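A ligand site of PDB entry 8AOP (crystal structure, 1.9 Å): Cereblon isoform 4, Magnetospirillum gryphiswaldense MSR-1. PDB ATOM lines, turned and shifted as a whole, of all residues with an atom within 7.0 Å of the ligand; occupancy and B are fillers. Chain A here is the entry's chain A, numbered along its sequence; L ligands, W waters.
The backbone NH (N) of Ala 52 is in hydrogen-bond range of the side-chain amide oxygen (OD1) of Asn 50, at 3.0 Å. The side-chain amide oxygen (OD1) of Asn 50 is in hydrogen-bond range of the backbone NH (N) of Gly 53. The indole nitrogen (NE1) of Trp 85 sits at hydrogen-bond distance from the backbone carbonyl oxygen (O) of Glu 76. O of Tyr 83 is in hydrogen-bond range of OG of Ser 78 (2.9 Å). The indole nitrogen (NE1) of Trp 79 sits at hydrogen-bond distance from the backbone carbonyl oxygen (O) of Phe 49, 2.9 Å away. The backbone carbonyl oxygen (O) of Ser 74 sits at hydrogen-bond distance from the backbone NH (N) of Trp 85 (2.7 Å). OG of Ser 78 sits at hydrogen-bond distance from O of Phe 80 (3.0 Å). OD1 of Asn 50 sits at hydrogen-bond distance from N of Met 54, at 3.0 Å.
Merely in contact with the ligand: Ser 78 (3.4 Å), Trp 99 (3.4 Å), Pro 51 (3.5 Å), Trp 85 (3.5 Å) and Asn 50 (3.7 Å). Hydrophobic or aromatic side chains within 4 Å of the ligand: Pro 51, Phe 77, Trp 79, Trp 85, Trp 99 and Tyr 101. Eight residues have an atom within 4 Å of the ligand: Asn 50, Pro 51, Phe 77, Ser 78, Trp 79, Trp 85, Trp 99 and Tyr 101.
O2 of the ligand lies within hydrogen-bond range of OH of Tyr 101, 2.8 Å away. N1 of the ligand lies within hydrogen-bond range of O of Phe 77 (2.8 Å). O2 of the ligand sits at hydrogen-bond distance from N of Trp 79, 3.0 Å away.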
ATOM      1  N   VAL A  48      -9.196 -19.312 -12.962  1.00  0.00           N
ATOM      2  CA  VAL A  48      -8.034 -18.968 -12.086  1.00  0.00           C
ATOM      3  C   VAL A  48      -6.750 -18.868 -12.926  1.00  0.00           C
ATOM      4  O   VAL A  48      -6.728 -19.429 -14.025  1.00  0.00           O
ATOM      5  CB  VAL A  48      -7.866 -20.010 -10.970  1.00  0.00           C
ATOM      6  CG1 VAL A  48      -9.071 -19.999 -10.024  1.00  0.00           C
ATOM      7  CG2 VAL A  48      -7.633 -21.399 -11.522  1.00  0.00           C
ATOM      8  N   PHE A  49      -5.732 -18.198 -12.383  1.00  0.00           N
ATOM      9  CA  PHE A  49      -4.395 -18.023 -12.994  1.00  0.00           C
ATOM     10  C   PHE A  49      -3.311 -18.433 -12.016  1.00  0.00           C
ATOM     11  O   PHE A  49      -3.395 -18.010 -10.853  1.00  0.00           O
ATOM     12  CB  PHE A  49      -4.124 -16.547 -13.329  1.00  0.00           C
ATOM     13  CG  PHE A  49      -4.947 -15.972 -14.438  1.00  0.00           C
ATOM     14  CD1 PHE A  49      -4.552 -16.118 -15.765  1.00  0.00           C
ATOM     15  CD2 PHE A  49      -6.079 -15.226 -14.159  1.00  0.00           C
ATOM     16  CE1 PHE A  49      -5.294 -15.563 -16.790  1.00  0.00           C
ATOM     17  CE2 PHE A  49      -6.812 -14.650 -15.193  1.00  0.00           C
ATOM     18  CZ  PHE A  49      -6.424 -14.829 -16.504  1.00  0.00           C
ATOM     19  N   ASN A  50      -2.291 -19.145 -12.497  1.00  0.00           N
ATOM     20  CA  ASN A  50      -1.098 -19.499 -11.680  1.00  0.00           C
ATOM     21  C   ASN A  50      -0.068 -18.376 -11.798  1.00  0.00           C
ATOM     22  O   ASN A  50      -0.237 -17.443 -12.578  1.00  0.00           O
ATOM     23  CB  ASN A  50      -0.626 -20.915 -12.021  1.00  0.00           C
ATOM     24  CG  ASN A  50       0.097 -21.024 -13.348  1.00  0.00           C
ATOM     25  OD1 ASN A  50       0.391 -20.024 -13.992  1.00  0.00           O
ATOM     26  ND2 ASN A  50       0.418 -22.253 -13.732  1.00  0.00           N
ATOM     27  N   PRO A  51       1.001 -18.398 -10.962  1.00  0.00           N
ATOM     28  CA  PRO A  51       2.019 -17.353 -11.013  1.00  0.00           C
ATOM     29  C   PRO A  51       2.751 -17.238 -12.349  1.00  0.00           C
ATOM     30  O   PRO A  51       3.309 -16.203 -12.580  1.00  0.00           O
ATOM     31  CB  PRO A  51       2.992 -17.754  -9.889  1.00  0.00           C
ATOM     32  CG  PRO A  51       2.159 -18.604  -8.939  1.00  0.00           C
ATOM     33  CD  PRO A  51       1.198 -19.346  -9.850  1.00  0.00           C
ATOM     34  N   ALA A  52       2.729 -18.280 -13.173  1.00  0.00           N
ATOM     35  CA  ALA A  52       3.317 -18.294 -14.534  1.00  0.00           C
ATOM     36  C   ALA A  52       2.345 -17.663 -15.560  1.00  0.00           C
ATOM     37  O   ALA A  52       2.747 -17.521 -16.778  1.00  0.00           O
ATOM     38  CB  ALA A  52       3.695 -19.714 -14.899  1.00  0.00           C
ATOM     39  N   GLY A  53       1.144 -17.259 -15.089  1.00  0.00           N
ATOM     40  CA  GLY A  53       0.130 -16.519 -15.877  1.00  0.00           C
ATOM     41  C   GLY A  53      -0.795 -17.429 -16.663  1.00  0.00           C
ATOM     42  O   GLY A  53      -1.666 -16.895 -17.372  1.00  0.00           O
ATOM     43  N   MET A  54      -0.661 -18.758 -16.534  1.00  0.00           N
ATOM     44  CA  MET A  54      -1.566 -19.716 -17.241  1.00  0.00           C
ATOM     45  C   MET A  54      -2.965 -19.611 -16.638  1.00  0.00           C
ATOM     46  O   MET A  54      -3.081 -19.591 -15.387  1.00  0.00           O
ATOM     47  CB  MET A  54      -1.109 -21.172 -17.119  1.00  0.00           C
ATOM     48  CG  MET A  54       0.345 -21.442 -17.421  1.00  0.00           C
ATOM     49  SD  MET A  54       0.655 -23.217 -17.480  1.00  0.00           S
ATOM     50  CE  MET A  54       0.368 -23.559 -19.219  1.00  0.00           C
ATOM     51  N   PHE A  56      -6.729 -21.286 -16.101  1.00  0.00           N
ATOM     52  CA  PHE A  56      -7.401 -22.599 -16.018  1.00  0.00           C
ATOM     53  C   PHE A  56      -8.872 -22.344 -15.736  1.00  0.00           C
ATOM     54  O   PHE A  56      -9.182 -21.532 -14.841  1.00  0.00           O
ATOM     55  CB  PHE A  56      -6.784 -23.466 -14.926  1.00  0.00           C
ATOM     56  CG  PHE A  56      -5.307 -23.715 -15.067  1.00  0.00           C
ATOM     57  CD1 PHE A  56      -4.826 -24.762 -15.840  1.00  0.00           C
ATOM     58  CD2 PHE A  56      -4.387 -22.917 -14.418  1.00  0.00           C
ATOM     59  CE1 PHE A  56      -3.469 -24.984 -15.963  1.00  0.00           C
ATOM     60  CE2 PHE A  56      -3.028 -23.151 -14.533  1.00  0.00           C
ATOM     61  CZ  PHE A  56      -2.568 -24.204 -15.284  1.00  0.00           C
ATOM     62  N   SER A  74       0.920 -28.346  -0.415  1.00  0.00           N
ATOM     63  CA  SER A  74       1.442 -26.953  -0.283  1.00  0.00           C
ATOM     64  C   SER A  74       0.275 -25.971  -0.196  1.00  0.00           C
ATOM     65  O   SER A  74      -0.697 -26.145  -0.937  1.00  0.00           O
ATOM     66  CB  SER A  74       2.339 -26.596  -1.443  1.00  0.00           C
ATOM     67  OG  SER A  74       2.785 -25.257  -1.313  1.00  0.00           O
ATOM     68  N   GLY A  75       0.388 -24.955   0.661  1.00  0.00           N
ATOM     69  CA  GLY A  75      -0.577 -23.833   0.791  1.00  0.00           C
ATOM     70  C   GLY A  75      -0.227 -22.663  -0.116  1.00  0.00           C
ATOM     71  O   GLY A  75      -1.059 -21.798  -0.265  1.00  0.00           O
ATOM     72  N   GLU A  76       0.967 -22.656  -0.723  1.00  0.00           N
ATOM     73  CA  GLU A  76       1.494 -21.503  -1.509  1.00  0.00           C
ATOM     74  C   GLU A  76       0.617 -21.283  -2.758  1.00  0.00           C
ATOM     75  O   GLU A  76       0.370 -22.245  -3.484  1.00  0.00           O
ATOM     76  CB  GLU A  76       2.964 -21.731  -1.870  1.00  0.00           C
ATOM     77  CG  GLU A  76       3.810 -21.938  -0.621  1.00  0.00           C
ATOM     78  CD  GLU A  76       5.316 -21.785  -0.757  1.00  0.00           C
ATOM     79  OE1 GLU A  76       5.833 -21.956  -1.883  1.00  0.00           O
ATOM     80  OE2 GLU A  76       5.961 -21.487   0.283  1.00  0.00           O
ATOM     81  N   PHE A  77       0.126 -20.059  -2.948  1.00  0.00           N
ATOM     82  CA  PHE A  77      -0.652 -19.604  -4.124  1.00  0.00           C
ATOM     83  C   PHE A  77      -1.989 -20.358  -4.220  1.00  0.00           C
ATOM     84  O   PHE A  77      -2.566 -20.367  -5.323  1.00  0.00           O
ATOM     85  CB  PHE A  77       0.152 -19.801  -5.408  1.00  0.00           C
ATOM     86  CG  PHE A  77       1.518 -19.170  -5.394  1.00  0.00           C
ATOM     87  CD1 PHE A  77       1.667 -17.788  -5.289  1.00  0.00           C
ATOM     88  CD2 PHE A  77       2.662 -19.944  -5.452  1.00  0.00           C
ATOM     89  CE1 PHE A  77       2.924 -17.214  -5.247  1.00  0.00           C
ATOM     90  CE2 PHE A  77       3.924 -19.365  -5.417  1.00  0.00           C
ATOM     91  CZ  PHE A  77       4.045 -17.995  -5.311  1.00  0.00           C
ATOM     92  N   SER A  78      -2.496 -20.957  -3.143  1.00  0.00           N
ATOM     93  CA  SER A  78      -3.774 -21.711  -3.214  1.00  0.00           C
ATOM     94  C   SER A  78      -4.890 -20.778  -3.686  1.00  0.00           C
ATOM     95  O   SER A  78      -5.039 -19.715  -3.111  1.00  0.00           O
ATOM     96  CB  SER A  78      -4.160 -22.375  -1.920  1.00  0.00           C
ATOM     97  OG  SER A  78      -5.367 -23.093  -2.136  1.00  0.00           O
ATOM     98  N   TRP A  79      -5.669 -21.209  -4.680  1.00  0.00           N
ATOM     99  CA  TRP A  79      -6.858 -20.463  -5.179  1.00  0.00           C
ATOM    100  C   TRP A  79      -8.018 -20.572  -4.194  1.00  0.00           C
ATOM    101  O   TRP A  79      -9.000 -19.828  -4.354  1.00  0.00           O
ATOM    102  CB  TRP A  79      -7.275 -21.000  -6.530  1.00  0.00           C
ATOM    103  CG  TRP A  79      -6.255 -20.761  -7.599  1.00  0.00           C
ATOM    104  CD1 TRP A  79      -5.616 -19.586  -7.881  1.00  0.00           C
ATOM    105  CD2 TRP A  79      -5.773 -21.727  -8.538  1.00  0.00           C
ATOM    106  NE1 TRP A  79      -4.783 -19.756  -8.955  1.00  0.00           N
ATOM    107  CE2 TRP A  79      -4.864 -21.050  -9.392  1.00  0.00           C
ATOM    108  CE3 TRP A  79      -6.023 -23.092  -8.767  1.00  0.00           C
ATOM    109  CZ2 TRP A  79      -4.200 -21.707 -10.427  1.00  0.00           C
ATOM    110  CZ3 TRP A  79      -5.379 -23.726  -9.802  1.00  0.00           C
ATOM    111  CH2 TRP A  79      -4.481 -23.033 -10.614  1.00  0.00           C
ATOM    112  N   PHE A  80      -7.932 -21.472  -3.222  1.00  0.00           N
ATOM    113  CA  PHE A  80      -9.043 -21.779  -2.296  1.00  0.00           C
ATOM    114  C   PHE A  80      -8.517 -21.614  -0.878  1.00  0.00           C
ATOM    115  O   PHE A  80      -7.711 -22.435  -0.411  1.00  0.00           O
ATOM    116  CB  PHE A  80      -9.620 -23.155  -2.604  1.00  0.00           C
ATOM    117  CG  PHE A  80     -10.110 -23.329  -4.015  1.00  0.00           C
ATOM    118  CD1 PHE A  80     -11.369 -22.886  -4.393  1.00  0.00           C
ATOM    119  CD2 PHE A  80      -9.329 -23.961  -4.971  1.00  0.00           C
ATOM    120  CE1 PHE A  80     -11.850 -23.091  -5.684  1.00  0.00           C
ATOM    121  CE2 PHE A  80      -9.800 -24.156  -6.263  1.00  0.00           C
ATOM    122  CZ  PHE A  80     -11.058 -23.713  -6.612  1.00  0.00           C
ATOM    123  N   TYR A  83      -7.059 -24.194   2.065  1.00  0.00           N
ATOM    124  CA  TYR A  83      -6.745 -25.498   1.443  1.00  0.00           C
ATOM    125  C   TYR A  83      -5.310 -25.530   0.935  1.00  0.00           C
ATOM    126  O   TYR A  83      -4.844 -24.537   0.348  1.00  0.00           O
ATOM    127  CB  TYR A  83      -7.693 -25.839   0.297  1.00  0.00           C
ATOM    128  CG  TYR A  83      -9.124 -26.044   0.693  1.00  0.00           C
ATOM    129  CD1 TYR A  83      -9.586 -27.289   1.105  1.00  0.00           C
ATOM    130  CD2 TYR A  83     -10.018 -24.993   0.668  1.00  0.00           C
ATOM    131  CE1 TYR A  83     -10.904 -27.474   1.483  1.00  0.00           C
ATOM    132  CE2 TYR A  83     -11.343 -25.171   1.031  1.00  0.00           C
ATOM    133  CZ  TYR A  83     -11.783 -26.408   1.449  1.00  0.00           C
ATOM    134  OH  TYR A  83     -13.101 -26.554   1.783  1.00  0.00           O
ATOM    135  N   TRP A  85      -2.700 -27.870  -1.615  1.00  0.00           N
ATOM    136  CA  TRP A  85      -2.917 -28.591  -2.889  1.00  0.00           C
ATOM    137  C   TRP A  85      -1.769 -29.577  -3.138  1.00  0.00           C
ATOM    138  O   TRP A  85      -0.636 -29.341  -2.682  1.00  0.00           O
ATOM    139  CB  TRP A  85      -3.108 -27.624  -4.065  1.00  0.00           C
ATOM    140  CG  TRP A  85      -2.019 -26.610  -4.182  1.00  0.00           C
ATOM    141  CD1 TRP A  85      -2.028 -25.356  -3.641  1.00  0.00           C
ATOM    142  CD2 TRP A  85      -0.736 -26.779  -4.821  1.00  0.00           C
ATOM    143  NE1 TRP A  85      -0.849 -24.731  -3.916  1.00  0.00           N
ATOM    144  CE2 TRP A  85      -0.028 -25.568  -4.618  1.00  0.00           C
ATOM    145  CE3 TRP A  85      -0.105 -27.827  -5.493  1.00  0.00           C
ATOM    146  CZ2 TRP A  85       1.261 -25.382  -5.108  1.00  0.00           C
ATOM    147  CZ3 TRP A  85       1.165 -27.630  -5.989  1.00  0.00           C
ATOM    148  CH2 TRP A  85       1.837 -26.412  -5.807  1.00  0.00           C
ATOM    149  N   THR A  86      -2.076 -30.632  -3.880  1.00  0.00           N
ATOM    150  CA  THR A  86      -1.089 -31.562  -4.485  1.00  0.00           C
ATOM    151  C   THR A  86      -1.460 -31.683  -5.960  1.00  0.00           C
ATOM    152  O   THR A  86      -2.648 -31.633  -6.270  1.00  0.00           O
ATOM    153  CB  THR A  86      -1.079 -32.919  -3.783  1.00  0.00           C
ATOM    154  OG1 THR A  86      -2.337 -33.536  -3.973  1.00  0.00           O
ATOM    155  CG2 THR A  86      -0.806 -32.806  -2.311  1.00  0.00           C
ATOM    156  N   ILE A  87      -0.464 -31.773  -6.839  1.00  0.00           N
ATOM    157  CA  ILE A  87      -0.701 -31.989  -8.294  1.00  0.00           C
ATOM    158  C   ILE A  87      -1.361 -33.358  -8.465  1.00  0.00           C
ATOM    159  O   ILE A  87      -0.899 -34.352  -7.822  1.00  0.00           O
ATOM    160  CB  ILE A  87       0.614 -31.834  -9.081  1.00  0.00           C
ATOM    161  CG1 ILE A  87       1.077 -30.373  -9.041  1.00  0.00           C
ATOM    162  CG2 ILE A  87       0.465 -32.347 -10.508  1.00  0.00           C
ATOM    163  CD1 ILE A  87       2.556 -30.191  -9.326  1.00  0.00           C
ATOM    164  N   HIS A  96      -1.426 -33.865 -16.750  1.00  0.00           N
ATOM    165  CA  HIS A  96      -1.761 -33.022 -15.572  1.00  0.00           C
ATOM    166  C   HIS A  96      -3.241 -32.628 -15.656  1.00  0.00           C
ATOM    167  O   HIS A  96      -3.611 -31.795 -16.508  1.00  0.00           O
ATOM    168  CB  HIS A  96      -0.818 -31.816 -15.470  1.00  0.00           C
ATOM    169  CG  HIS A  96      -1.206 -30.939 -14.333  1.00  0.00           C
ATOM    170  ND1 HIS A  96      -1.043 -29.573 -14.363  1.00  0.00           N
ATOM    171  CD2 HIS A  96      -1.795 -31.235 -13.145  1.00  0.00           C
ATOM    172  CE1 HIS A  96      -1.477 -29.059 -13.232  1.00  0.00           C
ATOM    173  NE2 HIS A  96      -1.952 -30.059 -12.468  1.00  0.00           N
ATOM    174  N   TRP A  99      -5.645 -30.645  -9.461  1.00  0.00           N
ATOM    175  CA  TRP A  99      -5.094 -30.618  -8.081  1.00  0.00           C
ATOM    176  C   TRP A  99      -6.076 -31.280  -7.132  1.00  0.00           C
ATOM    177  O   TRP A  99      -7.298 -31.152  -7.337  1.00  0.00           O
ATOM    178  CB  TRP A  99      -4.786 -29.175  -7.659  1.00  0.00           C
ATOM    179  CG  TRP A  99      -3.862 -28.458  -8.600  1.00  0.00           C
ATOM    180  CD1 TRP A  99      -2.505 -28.397  -8.528  1.00  0.00           C
ATOM    181  CD2 TRP A  99      -4.227 -27.754  -9.795  1.00  0.00           C
ATOM    182  NE1 TRP A  99      -2.003 -27.696  -9.587  1.00  0.00           N
ATOM    183  CE2 TRP A  99      -3.033 -27.278 -10.377  1.00  0.00           C
ATOM    184  CE3 TRP A  99      -5.446 -27.464 -10.438  1.00  0.00           C
ATOM    185  CZ2 TRP A  99      -3.011 -26.550 -11.566  1.00  0.00           C
ATOM    186  CZ3 TRP A  99      -5.427 -26.752 -11.613  1.00  0.00           C
ATOM    187  CH2 TRP A  99      -4.229 -26.299 -12.165  1.00  0.00           C
ATOM    188  N   TYR A 101      -7.160 -30.872  -3.182  1.00  0.00           N
ATOM    189  CA  TYR A 101      -7.143 -29.888  -2.087  1.00  0.00           C
ATOM    190  C   TYR A 101      -7.476 -30.611  -0.793  1.00  0.00           C
ATOM    191  O   TYR A 101      -8.358 -31.508  -0.831  1.00  0.00           O
ATOM    192  CB  TYR A 101      -8.085 -28.732  -2.390  1.00  0.00           C
ATOM    193  CG  TYR A 101      -7.605 -27.875  -3.532  1.00  0.00           C
ATOM    194  CD1 TYR A 101      -6.726 -26.834  -3.330  1.00  0.00           C
ATOM    195  CD2 TYR A 101      -8.003 -28.141  -4.831  1.00  0.00           C
ATOM    196  CE1 TYR A 101      -6.280 -26.035  -4.369  1.00  0.00           C
ATOM    197  CE2 TYR A 101      -7.586 -27.355  -5.882  1.00  0.00           C
ATOM    198  CZ  TYR A 101      -6.713 -26.305  -5.666  1.00  0.00           C
ATOM    199  OH  TYR A 101      -6.249 -25.530  -6.719  1.00  0.00           O
HETATM  200  N1  LIG L   1      -2.836 -22.451  -7.245  1.00  0.00           N
HETATM  201  C1  LIG L   1      -3.471 -23.595  -6.794  1.00  0.00           C
HETATM  202  C2  LIG L   1      -2.950 -24.901  -7.318  1.00  0.00           C
HETATM  203  C3  LIG L   1       0.136 -23.622  -9.244  1.00  0.00           C
HETATM  204  C4  LIG L   1       2.679 -22.568  -9.263  1.00  0.00           C
HETATM  205  C5  LIG L   1       2.576 -22.945 -10.605  1.00  0.00           C
HETATM  206  C6  LIG L   1       4.627 -21.783 -11.090  1.00  0.00           C
HETATM  207  C7  LIG L   1      -1.498 -24.838  -7.746  1.00  0.00           C
HETATM  208  C8  LIG L   1      -1.288 -23.687  -8.718  1.00  0.00           C
HETATM  209  C9  LIG L   1      -1.789 -22.389  -8.131  1.00  0.00           C
HETATM  210  S1  LIG L   1       1.429 -23.052  -8.105  1.00  0.00           S
HETATM  211  O1  LIG L   1      -1.319 -21.325  -8.459  1.00  0.00           O
HETATM  212  O2  LIG L   1      -4.428 -23.537  -6.044  1.00  0.00           O
HETATM  213  C10 LIG L   1       3.556 -22.554 -11.515  1.00  0.00           C
HETATM  214  C11 LIG L   1       4.745 -21.392  -9.757  1.00  0.00           C
HETATM  215  C12 LIG L   1       3.765 -21.783  -8.847  1.00  0.00           C
HETATM  216  N2  LIG L   1       5.821 -20.629  -9.361  1.00  0.00           N
HETATM  217  O   HOH W   1      -0.166 -25.134 -12.376  1.00  0.00           O
